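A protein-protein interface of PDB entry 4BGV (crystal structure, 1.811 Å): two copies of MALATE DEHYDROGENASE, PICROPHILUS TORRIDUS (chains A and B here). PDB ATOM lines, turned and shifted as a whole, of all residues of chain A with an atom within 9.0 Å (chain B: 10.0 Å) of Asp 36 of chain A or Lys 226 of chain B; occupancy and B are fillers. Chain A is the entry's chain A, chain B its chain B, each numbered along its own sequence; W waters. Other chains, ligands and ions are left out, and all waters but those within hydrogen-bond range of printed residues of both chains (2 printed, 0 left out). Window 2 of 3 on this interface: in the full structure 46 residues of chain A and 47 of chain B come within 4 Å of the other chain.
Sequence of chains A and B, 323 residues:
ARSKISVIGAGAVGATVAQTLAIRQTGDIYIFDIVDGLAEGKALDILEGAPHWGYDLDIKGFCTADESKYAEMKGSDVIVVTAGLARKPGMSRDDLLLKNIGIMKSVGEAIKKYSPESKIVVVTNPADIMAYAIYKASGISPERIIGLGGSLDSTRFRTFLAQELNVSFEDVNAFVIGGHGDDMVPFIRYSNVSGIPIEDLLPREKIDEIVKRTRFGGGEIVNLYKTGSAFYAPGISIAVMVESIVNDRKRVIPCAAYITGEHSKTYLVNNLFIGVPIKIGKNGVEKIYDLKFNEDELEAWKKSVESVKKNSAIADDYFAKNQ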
ATOM      1  N   ALA A  10       3.248  -4.004  -4.068  1.00  0.00           N
ATOM      2  CA  ALA A  10       4.210  -3.665  -3.023  1.00  0.00           C
ATOM      3  C   ALA A  10       4.541  -2.173  -2.984  1.00  0.00           C
ATOM      4  O   ALA A  10       5.579  -1.777  -2.466  1.00  0.00           O
ATOM      5  CB  ALA A  10       5.483  -4.503  -3.177  1.00  0.00           C
ATOM      6  N   PHE A  32       3.687  -9.509  -3.368  1.00  0.00           N
ATOM      7  CA  PHE A  32       3.921  -9.694  -4.803  1.00  0.00           C
ATOM      8  C   PHE A  32       3.896  -8.361  -5.550  1.00  0.00           C
ATOM      9  O   PHE A  32       3.061  -7.501  -5.275  1.00  0.00           O
ATOM     10  CB  PHE A  32       2.858 -10.631  -5.404  1.00  0.00           C
ATOM     11  CG  PHE A  32       2.823 -11.991  -4.754  1.00  0.00           C
ATOM     12  CD1 PHE A  32       2.162 -12.182  -3.538  1.00  0.00           C
ATOM     13  CD2 PHE A  32       3.472 -13.067  -5.342  1.00  0.00           C
ATOM     14  CE1 PHE A  32       2.156 -13.428  -2.919  1.00  0.00           C
ATOM     15  CE2 PHE A  32       3.460 -14.320  -4.745  1.00  0.00           C
ATOM     16  CZ  PHE A  32       2.801 -14.505  -3.525  1.00  0.00           C
ATOM     17  N   ASP A  33       4.815  -8.199  -6.499  1.00  0.00           N
ATOM     18  CA  ASP A  33       4.844  -7.011  -7.338  1.00  0.00           C
ATOM     19  C   ASP A  33       5.589  -7.301  -8.634  1.00  0.00           C
ATOM     20  O   ASP A  33       6.583  -8.038  -8.656  1.00  0.00           O
ATOM     21  CB  ASP A  33       5.486  -5.816  -6.624  1.00  0.00           C
ATOM     22  CG  ASP A  33       5.059  -4.480  -7.237  1.00  0.00           C
ATOM     23  OD1 ASP A  33       5.594  -4.118  -8.304  1.00  0.00           O
ATOM     24  OD2 ASP A  33       4.156  -3.814  -6.684  1.00  0.00           O
ATOM     25  N   ILE A  34       5.102  -6.701  -9.715  1.00  0.00           N
ATOM     26  CA  ILE A  34       5.672  -6.906 -11.030  1.00  0.00           C
ATOM     27  C   ILE A  34       7.030  -6.214 -11.181  1.00  0.00           C
ATOM     28  O   ILE A  34       7.819  -6.571 -12.056  1.00  0.00           O
ATOM     29  CB  ILE A  34       4.695  -6.391 -12.128  1.00  0.00           C
ATOM     30  CG1 ILE A  34       5.147  -6.827 -13.520  1.00  0.00           C
ATOM     31  CG2 ILE A  34       4.546  -4.881 -12.047  1.00  0.00           C
ATOM     32  CD1 ILE A  34       4.330  -7.970 -14.088  1.00  0.00           C
ATOM     33  N   VAL A  35       7.310  -5.239 -10.321  1.00  0.00           N
ATOM     34  CA  VAL A  35       8.584  -4.527 -10.376  1.00  0.00           C
ATOM     35  C   VAL A  35       9.694  -5.327  -9.697  1.00  0.00           C
ATOM     36  O   VAL A  35       9.601  -5.638  -8.522  1.00  0.00           O
ATOM     37  CB  VAL A  35       8.476  -3.143  -9.719  1.00  0.00           C
ATOM     38  CG1 VAL A  35       9.840  -2.458  -9.673  1.00  0.00           C
ATOM     39  CG2 VAL A  35       7.472  -2.286 -10.480  1.00  0.00           C
ATOM     40  N   ASP A  36      10.750  -5.648 -10.443  1.00  0.00           N
ATOM     41  CA  ASP A  36      11.816  -6.498  -9.911  1.00  0.00           C
ATOM     42  C   ASP A  36      12.457  -5.894  -8.659  1.00  0.00           C
ATOM     43  O   ASP A  36      12.835  -4.723  -8.638  1.00  0.00           O
ATOM     44  CB  ASP A  36      12.878  -6.785 -10.975  1.00  0.00           C
ATOM     45  CG  ASP A  36      13.895  -7.819 -10.516  1.00  0.00           C
ATOM     46  OD1 ASP A  36      13.490  -8.843  -9.917  1.00  0.00           O
ATOM     47  OD2 ASP A  36      15.102  -7.597 -10.744  1.00  0.00           O
ATOM     48  N   GLY A  37      12.545  -6.702  -7.608  1.00  0.00           N
ATOM     49  CA  GLY A  37      13.170  -6.294  -6.364  1.00  0.00           C
ATOM     50  C   GLY A  37      12.254  -5.654  -5.330  1.00  0.00           C
ATOM     51  O   GLY A  37      12.565  -5.675  -4.141  1.00  0.00           O
ATOM     52  N   LEU A  38      11.143  -5.066  -5.773  1.00  0.00           N
ATOM     53  CA  LEU A  38      10.331  -4.216  -4.893  1.00  0.00           C
ATOM     54  C   LEU A  38       9.660  -4.989  -3.770  1.00  0.00           C
ATOM     55  O   LEU A  38       9.792  -4.625  -2.601  1.00  0.00           O
ATOM     56  CB  LEU A  38       9.280  -3.413  -5.679  1.00  0.00           C
ATOM     57  CG  LEU A  38       8.449  -2.416  -4.851  1.00  0.00           C
ATOM     58  CD1 LEU A  38       9.359  -1.301  -4.312  1.00  0.00           C
ATOM     59  CD2 LEU A  38       7.301  -1.825  -5.696  1.00  0.00           C
ATOM     60  N   ALA A  39       8.939  -6.051  -4.114  1.00  0.00           N
ATOM     61  CA  ALA A  39       8.274  -6.845  -3.084  1.00  0.00           C
ATOM     62  C   ALA A  39       9.283  -7.541  -2.163  1.00  0.00           C
ATOM     63  O   ALA A  39       9.087  -7.583  -0.955  1.00  0.00           O
ATOM     64  CB  ALA A  39       7.328  -7.861  -3.698  1.00  0.00           C
ATOM     65  N   GLU A  40      10.351  -8.088  -2.733  1.00  0.00           N
ATOM     66  CA  GLU A  40      11.409  -8.691  -1.912  1.00  0.00           C
ATOM     67  C   GLU A  40      12.026  -7.655  -0.950  1.00  0.00           C
ATOM     68  O   GLU A  40      12.298  -7.950   0.227  1.00  0.00           O
ATOM     69  CB  GLU A  40      12.489  -9.316  -2.815  1.00  0.00           C
ATOM     70  CG  GLU A  40      13.731  -9.785  -2.085  1.00  0.00           C
ATOM     71  CD  GLU A  40      14.711 -10.528  -2.992  1.00  0.00           C
ATOM     72  OE1 GLU A  40      14.412 -10.691  -4.195  1.00  0.00           O
ATOM     73  OE2 GLU A  40      15.776 -10.954  -2.487  1.00  0.00           O
ATOM     74  N   GLY A  41      12.237  -6.441  -1.446  1.00  0.00           N
ATOM     75  CA  GLY A  41      12.798  -5.382  -0.625  1.00  0.00           C
ATOM     76  C   GLY A  41      11.863  -4.954   0.494  1.00  0.00           C
ATOM     77  O   GLY A  41      12.299  -4.787   1.640  1.00  0.00           O
ATOM     78  N   GLY A  61       8.864 -11.763  -0.223  1.00  0.00           N
ATOM     79  CA  GLY A  61       8.444 -10.993  -1.389  1.00  0.00           C
ATOM     80  C   GLY A  61       8.862 -11.641  -2.701  1.00  0.00           C
ATOM     81  O   GLY A  61       9.926 -12.255  -2.775  1.00  0.00           O
ATOM     82  N   PHE A  62       8.044 -11.480  -3.744  1.00  0.00           N
ATOM     83  CA  PHE A  62       8.281 -12.150  -5.016  1.00  0.00           C
ATOM     84  C   PHE A  62       8.024 -11.219  -6.190  1.00  0.00           C
ATOM     85  O   PHE A  62       7.137 -10.367  -6.118  1.00  0.00           O
ATOM     86  CB  PHE A  62       7.364 -13.368  -5.136  1.00  0.00           C
ATOM     87  CG  PHE A  62       7.562 -14.372  -4.048  1.00  0.00           C
ATOM     88  CD1 PHE A  62       8.561 -15.332  -4.151  1.00  0.00           C
ATOM     89  CD2 PHE A  62       6.777 -14.329  -2.900  1.00  0.00           C
ATOM     90  CE1 PHE A  62       8.762 -16.265  -3.134  1.00  0.00           C
ATOM     91  CE2 PHE A  62       6.968 -15.249  -1.881  1.00  0.00           C
ATOM     92  CZ  PHE A  62       7.960 -16.220  -2.000  1.00  0.00           C
ATOM     93  N   CYS A  63       8.782 -11.396  -7.271  1.00  0.00           N
ATOM     94  CA  CYS A  63       8.566 -10.614  -8.483  1.00  0.00           C
ATOM     95  C   CYS A  63       7.634 -11.361  -9.430  1.00  0.00           C
ATOM     96  O   CYS A  63       7.892 -12.511  -9.785  1.00  0.00           O
ATOM     97  CB  CYS A  63       9.891 -10.293  -9.187  1.00  0.00           C
ATOM     98  SG  CYS A  63       9.675  -9.291 -10.679  1.00  0.00           S
ATOM     99  N   THR A  64       6.554 -10.705  -9.844  1.00  0.00           N
ATOM    100  CA  THR A  64       5.572 -11.345 -10.724  1.00  0.00           C
ATOM    101  C   THR A  64       5.695 -10.923 -12.189  1.00  0.00           C
ATOM    102  O   THR A  64       4.746 -11.086 -12.962  1.00  0.00           O
ATOM    103  CB  THR A  64       4.153 -11.078 -10.244  1.00  0.00           C
ATOM    104  OG1 THR A  64       3.994  -9.674 -10.017  1.00  0.00           O
ATOM    105  CG2 THR A  64       3.880 -11.850  -8.928  1.00  0.00           C
ATOM    106  N   ALA A  65       6.857 -10.382 -12.562  1.00  0.00           N
ATOM    107  CA  ALA A  65       7.170 -10.148 -13.978  1.00  0.00           C
ATOM    108  C   ALA A  65       6.877 -11.416 -14.779  1.00  0.00           C
ATOM    109  O   ALA A  65       6.355 -11.355 -15.895  1.00  0.00           O
ATOM    110  CB  ALA A  65       8.623  -9.730 -14.156  1.00  0.00           C
ATOM    111  N   ASP A  66       7.215 -12.564 -14.195  1.00  0.00           N
ATOM    112  CA  ASP A  66       6.710 -13.829 -14.688  1.00  0.00           C
ATOM    113  C   ASP A  66       5.572 -14.269 -13.774  1.00  0.00           C
ATOM    114  O   ASP A  66       5.731 -14.336 -12.550  1.00  0.00           O
ATOM    115  CB  ASP A  66       7.801 -14.893 -14.723  1.00  0.00           C
ATOM    116  CG  ASP A  66       7.401 -16.097 -15.551  1.00  0.00           C
ATOM    117  OD1 ASP A  66       6.568 -16.900 -15.076  1.00  0.00           O
ATOM    118  OD2 ASP A  66       7.902 -16.237 -16.686  1.00  0.00           O
ATOM    119  N   LYS A  69       5.364 -16.962 -10.642  1.00  0.00           N
ATOM    120  CA  LYS A  69       5.617 -16.629  -9.233  1.00  0.00           C
ATOM    121  C   LYS A  69       4.353 -16.527  -8.381  1.00  0.00           C
ATOM    122  O   LYS A  69       4.415 -16.664  -7.158  1.00  0.00           O
ATOM    123  CB  LYS A  69       6.446 -15.353  -9.116  1.00  0.00           C
ATOM    124  CG  LYS A  69       7.936 -15.595  -9.376  1.00  0.00           C
ATOM    125  CD  LYS A  69       8.591 -16.220  -8.164  1.00  0.00           C
ATOM    126  CE  LYS A  69       9.857 -16.959  -8.550  1.00  0.00           C
ATOM    127  NZ  LYS A  69      10.690 -16.155  -9.488  1.00  0.00           N
ATOM    128  N   ALA B  86      20.173  11.750   0.350  1.00  0.00           N
ATOM    129  CA  ALA B  86      20.825  10.510  -0.053  1.00  0.00           C
ATOM    130  C   ALA B  86      21.546  10.826  -1.358  1.00  0.00           C
ATOM    131  O   ALA B  86      21.268  11.851  -1.986  1.00  0.00           O
ATOM    132  CB  ALA B  86      19.814   9.403  -0.248  1.00  0.00           C
ATOM    133  N   ARG B  87      22.471   9.960  -1.763  1.00  0.00           N
ATOM    134  CA  ARG B  87      23.343  10.247  -2.904  1.00  0.00           C
ATOM    135  C   ARG B  87      22.611  10.644  -4.191  1.00  0.00           C
ATOM    136  O   ARG B  87      21.640  10.005  -4.594  1.00  0.00           O
ATOM    137  CB  ARG B  87      24.303   9.081  -3.174  1.00  0.00           C
ATOM    138  CG  ARG B  87      25.415   8.958  -2.147  1.00  0.00           C
ATOM    139  CD  ARG B  87      26.589   8.147  -2.673  1.00  0.00           C
ATOM    140  NE  ARG B  87      26.278   6.728  -2.810  1.00  0.00           N
ATOM    141  CZ  ARG B  87      27.175   5.797  -3.123  1.00  0.00           C
ATOM    142  NH1 ARG B  87      28.440   6.139  -3.329  1.00  0.00           N
ATOM    143  NH2 ARG B  87      26.810   4.526  -3.230  1.00  0.00           N
ATOM    144  N   PRO B  89      23.133  11.572  -8.440  1.00  0.00           N
ATOM    145  CA  PRO B  89      24.036  11.191  -9.532  1.00  0.00           C
ATOM    146  C   PRO B  89      25.245  12.117  -9.628  1.00  0.00           C
ATOM    147  O   PRO B  89      25.102  13.291  -9.973  1.00  0.00           O
ATOM    148  CB  PRO B  89      23.156  11.342 -10.775  1.00  0.00           C
ATOM    149  CG  PRO B  89      21.781  11.083 -10.280  1.00  0.00           C
ATOM    150  CD  PRO B  89      21.734  11.664  -8.894  1.00  0.00           C
ATOM    151  N   GLY B 218      22.224  -2.345   4.797  1.00  0.00           N
ATOM    152  CA  GLY B 218      21.555  -1.165   4.249  1.00  0.00           C
ATOM    153  C   GLY B 218      21.630  -1.164   2.734  1.00  0.00           C
ATOM    154  O   GLY B 218      20.642  -0.886   2.045  1.00  0.00           O
ATOM    155  N   GLY B 219      22.813  -1.476   2.212  1.00  0.00           N
ATOM    156  CA  GLY B 219      23.010  -1.588   0.780  1.00  0.00           C
ATOM    157  C   GLY B 219      22.207  -2.719   0.149  1.00  0.00           C
ATOM    158  O   GLY B 219      21.812  -2.625  -1.009  1.00  0.00           O
ATOM    159  N   GLU B 220      21.987  -3.797   0.896  1.00  0.00           N
ATOM    160  CA  GLU B 220      21.161  -4.900   0.388  1.00  0.00           C
ATOM    161  C   GLU B 220      19.749  -4.387   0.079  1.00  0.00           C
ATOM    162  O   GLU B 220      19.166  -4.724  -0.950  1.00  0.00           O
ATOM    163  CB  GLU B 220      21.107  -6.057   1.392  1.00  0.00           C
ATOM    164  CG  GLU B 220      20.209  -7.210   0.945  1.00  0.00           C
ATOM    165  CD  GLU B 220      20.213  -8.379   1.913  1.00  0.00           C
ATOM    166  OE1 GLU B 220      20.694  -8.220   3.063  1.00  0.00           O
ATOM    167  OE2 GLU B 220      19.718  -9.458   1.524  1.00  0.00           O
ATOM    168  N   ILE B 221      19.218  -3.554   0.971  1.00  0.00           N
ATOM    169  CA  ILE B 221      17.885  -2.987   0.774  1.00  0.00           C
ATOM    170  C   ILE B 221      17.879  -1.982  -0.380  1.00  0.00           C
ATOM    171  O   ILE B 221      16.966  -1.977  -1.217  1.00  0.00           O
ATOM    172  CB  ILE B 221      17.352  -2.345   2.078  1.00  0.00           C
ATOM    173  CG1 ILE B 221      17.238  -3.417   3.177  1.00  0.00           C
ATOM    174  CG2 ILE B 221      16.000  -1.694   1.844  1.00  0.00           C
ATOM    175  CD1 ILE B 221      16.245  -4.533   2.831  1.00  0.00           C
ATOM    176  N   VAL B 222      18.911  -1.143  -0.436  1.00  0.00           N
ATOM    177  CA  VAL B 222      19.045  -0.168  -1.517  1.00  0.00           C
ATOM    178  C   VAL B 222      19.049  -0.867  -2.877  1.00  0.00           C
ATOM    179  O   VAL B 222      18.385  -0.416  -3.806  1.00  0.00           O
ATOM    180  CB  VAL B 222      20.318   0.705  -1.360  1.00  0.00           C
ATOM    181  CG1 VAL B 222      20.618   1.469  -2.654  1.00  0.00           C
ATOM    182  CG2 VAL B 222      20.165   1.666  -0.190  1.00  0.00           C
ATOM    183  N   ASN B 223      19.756  -1.997  -2.978  1.00  0.00           N
ATOM    184  CA  ASN B 223      19.815  -2.740  -4.238  1.00  0.00           C
ATOM    185  C   ASN B 223      18.467  -3.355  -4.647  1.00  0.00           C
ATOM    186  O   ASN B 223      18.227  -3.616  -5.827  1.00  0.00           O
ATOM    187  CB  ASN B 223      20.907  -3.815  -4.193  1.00  0.00           C
ATOM    188  CG  ASN B 223      22.305  -3.227  -4.064  1.00  0.00           C
ATOM    189  OD1 ASN B 223      22.548  -2.073  -4.429  1.00  0.00           O
ATOM    190  ND2 ASN B 223      23.235  -4.026  -3.546  1.00  0.00           N
ATOM    191  N   LEU B 224      17.584  -3.568  -3.673  1.00  0.00           N
ATOM    192  CA  LEU B 224      16.246  -4.072  -3.965  1.00  0.00           C
ATOM    193  C   LEU B 224      15.262  -2.937  -4.295  1.00  0.00           C
ATOM    194  O   LEU B 224      14.505  -3.038  -5.261  1.00  0.00           O
ATOM    195  CB  LEU B 224      15.720  -4.929  -2.809  1.00  0.00           C
ATOM    196  CG  LEU B 224      16.462  -6.255  -2.600  1.00  0.00           C
ATOM    197  CD1 LEU B 224      16.120  -6.837  -1.244  1.00  0.00           C
ATOM    198  CD2 LEU B 224      16.125  -7.238  -3.709  1.00  0.00           C
ATOM    199  N   TYR B 225      15.265  -1.874  -3.494  1.00  0.00           N
ATOM    200  CA  TYR B 225      14.393  -0.721  -3.754  1.00  0.00           C
ATOM    201  C   TYR B 225      14.817   0.041  -5.018  1.00  0.00           C
ATOM    202  O   TYR B 225      13.985   0.651  -5.709  1.00  0.00           O
ATOM    203  CB  TYR B 225      14.389   0.245  -2.554  1.00  0.00           C
ATOM    204  CG  TYR B 225      13.593  -0.195  -1.318  1.00  0.00           C
ATOM    205  CD1 TYR B 225      12.653  -1.230  -1.372  1.00  0.00           C
ATOM    206  CD2 TYR B 225      13.784   0.442  -0.098  1.00  0.00           C
ATOM    207  CE1 TYR B 225      11.923  -1.615  -0.230  1.00  0.00           C
ATOM    208  CE2 TYR B 225      13.064   0.061   1.052  1.00  0.00           C
ATOM    209  CZ  TYR B 225      12.136  -0.964   0.976  1.00  0.00           C
ATOM    210  OH  TYR B 225      11.438  -1.311   2.122  1.00  0.00           O
ATOM    211  N   LYS B 226      16.121   0.011  -5.296  1.00  0.00           N
ATOM    212  CA  LYS B 226      16.733   0.699  -6.444  1.00  0.00           C
ATOM    213  C   LYS B 226      16.735   2.227  -6.368  1.00  0.00           C
ATOM    214  O   LYS B 226      17.721   2.853  -6.736  1.00  0.00           O
ATOM    215  CB  LYS B 226      16.141   0.222  -7.777  1.00  0.00           C
ATOM    216  CG  LYS B 226      16.181  -1.287  -7.920  1.00  0.00           C
ATOM    217  CD  LYS B 226      16.143  -1.741  -9.359  1.00  0.00           C
ATOM    218  CE  LYS B 226      16.000  -3.255  -9.437  1.00  0.00           C
ATOM    219  NZ  LYS B 226      16.799  -3.932  -8.377  1.00  0.00           N
ATOM    220  N   THR B 227      15.644   2.825  -5.898  1.00  0.00           N
ATOM    221  CA  THR B 227      15.530   4.281  -5.879  1.00  0.00           C
ATOM    222  C   THR B 227      15.393   4.888  -4.487  1.00  0.00           C
ATOM    223  O   THR B 227      15.178   6.091  -4.346  1.00  0.00           O
ATOM    224  CB  THR B 227      14.337   4.756  -6.719  1.00  0.00           C
ATOM    225  OG1 THR B 227      13.130   4.181  -6.198  1.00  0.00           O
ATOM    226  CG2 THR B 227      14.516   4.335  -8.165  1.00  0.00           C
ATOM    227  N   GLY B 228      15.507   4.065  -3.455  1.00  0.00           N
ATOM    228  CA  GLY B 228      15.397   4.577  -2.105  1.00  0.00           C
ATOM    229  C   GLY B 228      16.077   3.620  -1.157  1.00  0.00           C
ATOM    230  O   GLY B 228      16.602   2.599  -1.592  1.00  0.00           O
ATOM    231  N   SER B 229      16.067   3.940   0.131  1.00  0.00           N
ATOM    232  CA  SER B 229      16.723   3.091   1.110  1.00  0.00           C
ATOM    233  C   SER B 229      15.745   2.587   2.167  1.00  0.00           C
ATOM    234  O   SER B 229      14.567   2.962   2.170  1.00  0.00           O
ATOM    235  CB  SER B 229      17.879   3.831   1.777  1.00  0.00           C
ATOM    236  OG  SER B 229      17.431   5.046   2.332  1.00  0.00           O
ATOM    237  N   ALA B 230      16.258   1.742   3.059  1.00  0.00           N
ATOM    238  CA  ALA B 230      15.452   1.117   4.109  1.00  0.00           C
ATOM    239  C   ALA B 230      14.735   2.156   4.970  1.00  0.00           C
ATOM    240  O   ALA B 230      15.280   3.225   5.246  1.00  0.00           O
ATOM    241  CB  ALA B 230      16.348   0.222   5.001  1.00  0.00           C
ATOM    242  N   PHE B 231      13.520   1.829   5.415  1.00  0.00           N
ATOM    243  CA  PHE B 231      12.791   2.704   6.334  1.00  0.00           C
ATOM    244  C   PHE B 231      11.953   1.945   7.379  1.00  0.00           C
ATOM    245  O   PHE B 231      11.761   2.430   8.492  1.00  0.00           O
ATOM    246  CB  PHE B 231      11.938   3.736   5.583  1.00  0.00           C
ATOM    247  CG  PHE B 231      10.927   3.139   4.633  1.00  0.00           C
ATOM    248  CD1 PHE B 231      11.299   2.774   3.339  1.00  0.00           C
ATOM    249  CD2 PHE B 231       9.603   2.959   5.029  1.00  0.00           C
ATOM    250  CE1 PHE B 231      10.379   2.229   2.463  1.00  0.00           C
ATOM    251  CE2 PHE B 231       8.663   2.430   4.137  1.00  0.00           C
ATOM    252  CZ  PHE B 231       9.055   2.062   2.860  1.00  0.00           C
HETATM  253  O   HOH W   1      18.216  -9.818  -0.510  1.00  0.00           O
HETATM  254  O   HOH W   2      12.356  -2.433  -7.036  1.00  0.00           O
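Of chain B, only Lys 226 (3.6 Å) comes within 4 Å of Asp 36 of chain A. Printed residues of chain A within 4 Å of Lys 226 of chain B: Asp 36. Gly 37 of chain A touches just one residue of chain B: Leu 224. No residue of chain A comes within 4 Å of Thr 227 of chain B. Printed residues of chain B within 4 Å of Gly 41 of chain A: Leu 224 and Tyr 225. Printed residues of chain A within 4 Å of Leu 224 of chain B: Gly 37, Leu 38, Glu 40 and Gly 41. Of the printed residues of chain B, Leu 38 of chain A touches Leu 224. Of the printed residues of chain A, Tyr 225 of chain B touches Gly 41. Printed residues of chain B within 4 Å of Glu 40 of chain A: Leu 224. Gly 218 of chain B touches none of the printed residues of chain A. Ala 65 of chain A touches none of the printed residues of chain B. The nearest residue of chain A that does not touch Lys 226 of chain B is Gly 37 of chain A (4.8 Å). The nearest printed residue of chain B that does not touch Glu 40 of chain A is Glu 220 of chain B (5.8 Å).
Printed residues of chain B that touch a printed residue of chain A: Leu 224, Tyr 225 and Lys 226. Hydrophobic or aromatic side chains of chain B that line the printed part of chain A: Leu 224 and Tyr 225. Among the printed residues, no Asp or Glu carboxylate lies within 4 Å of a Lys or Arg side-chain nitrogen of the other chain.
No position is printed for both chains. Of the 6 pairs that touch across the chains among the printed residues, none has its exchanged pair printed and touching as well.
Water W1 bridges OE2 of Glu 220 of chain B and OE2 of Glu 40 of chain A. Water W2 lies within hydrogen-bond range of O of Asp 36 of chain A (2.8 Å), O of Leu 224 of chain B (2.9 Å) and N of Leu 38 of chain A (3.2 Å).
Among the printed residues, merely in contact across the chains: Asp 36 of chain A with Lys 226 of chain B, Leu 38 of chain A with Leu 224 of chain B, Glu 40 of chain A with Leu 224 of chain B, Gly 41 of chain A with Leu 224 of chain B and Gly 41 of chain A with Tyr 225 of chain B.
The backbone carbonyl oxygen (O) of Gly 37 of chain A lies close to the backbone carbonyl oxygen (O) of Leu 224 of chain B, 3.5 Å away.
NZ of Lys 226 of chain B is in hydrogen-bond range of O of Asn 223 of chain B (2.9 Å).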
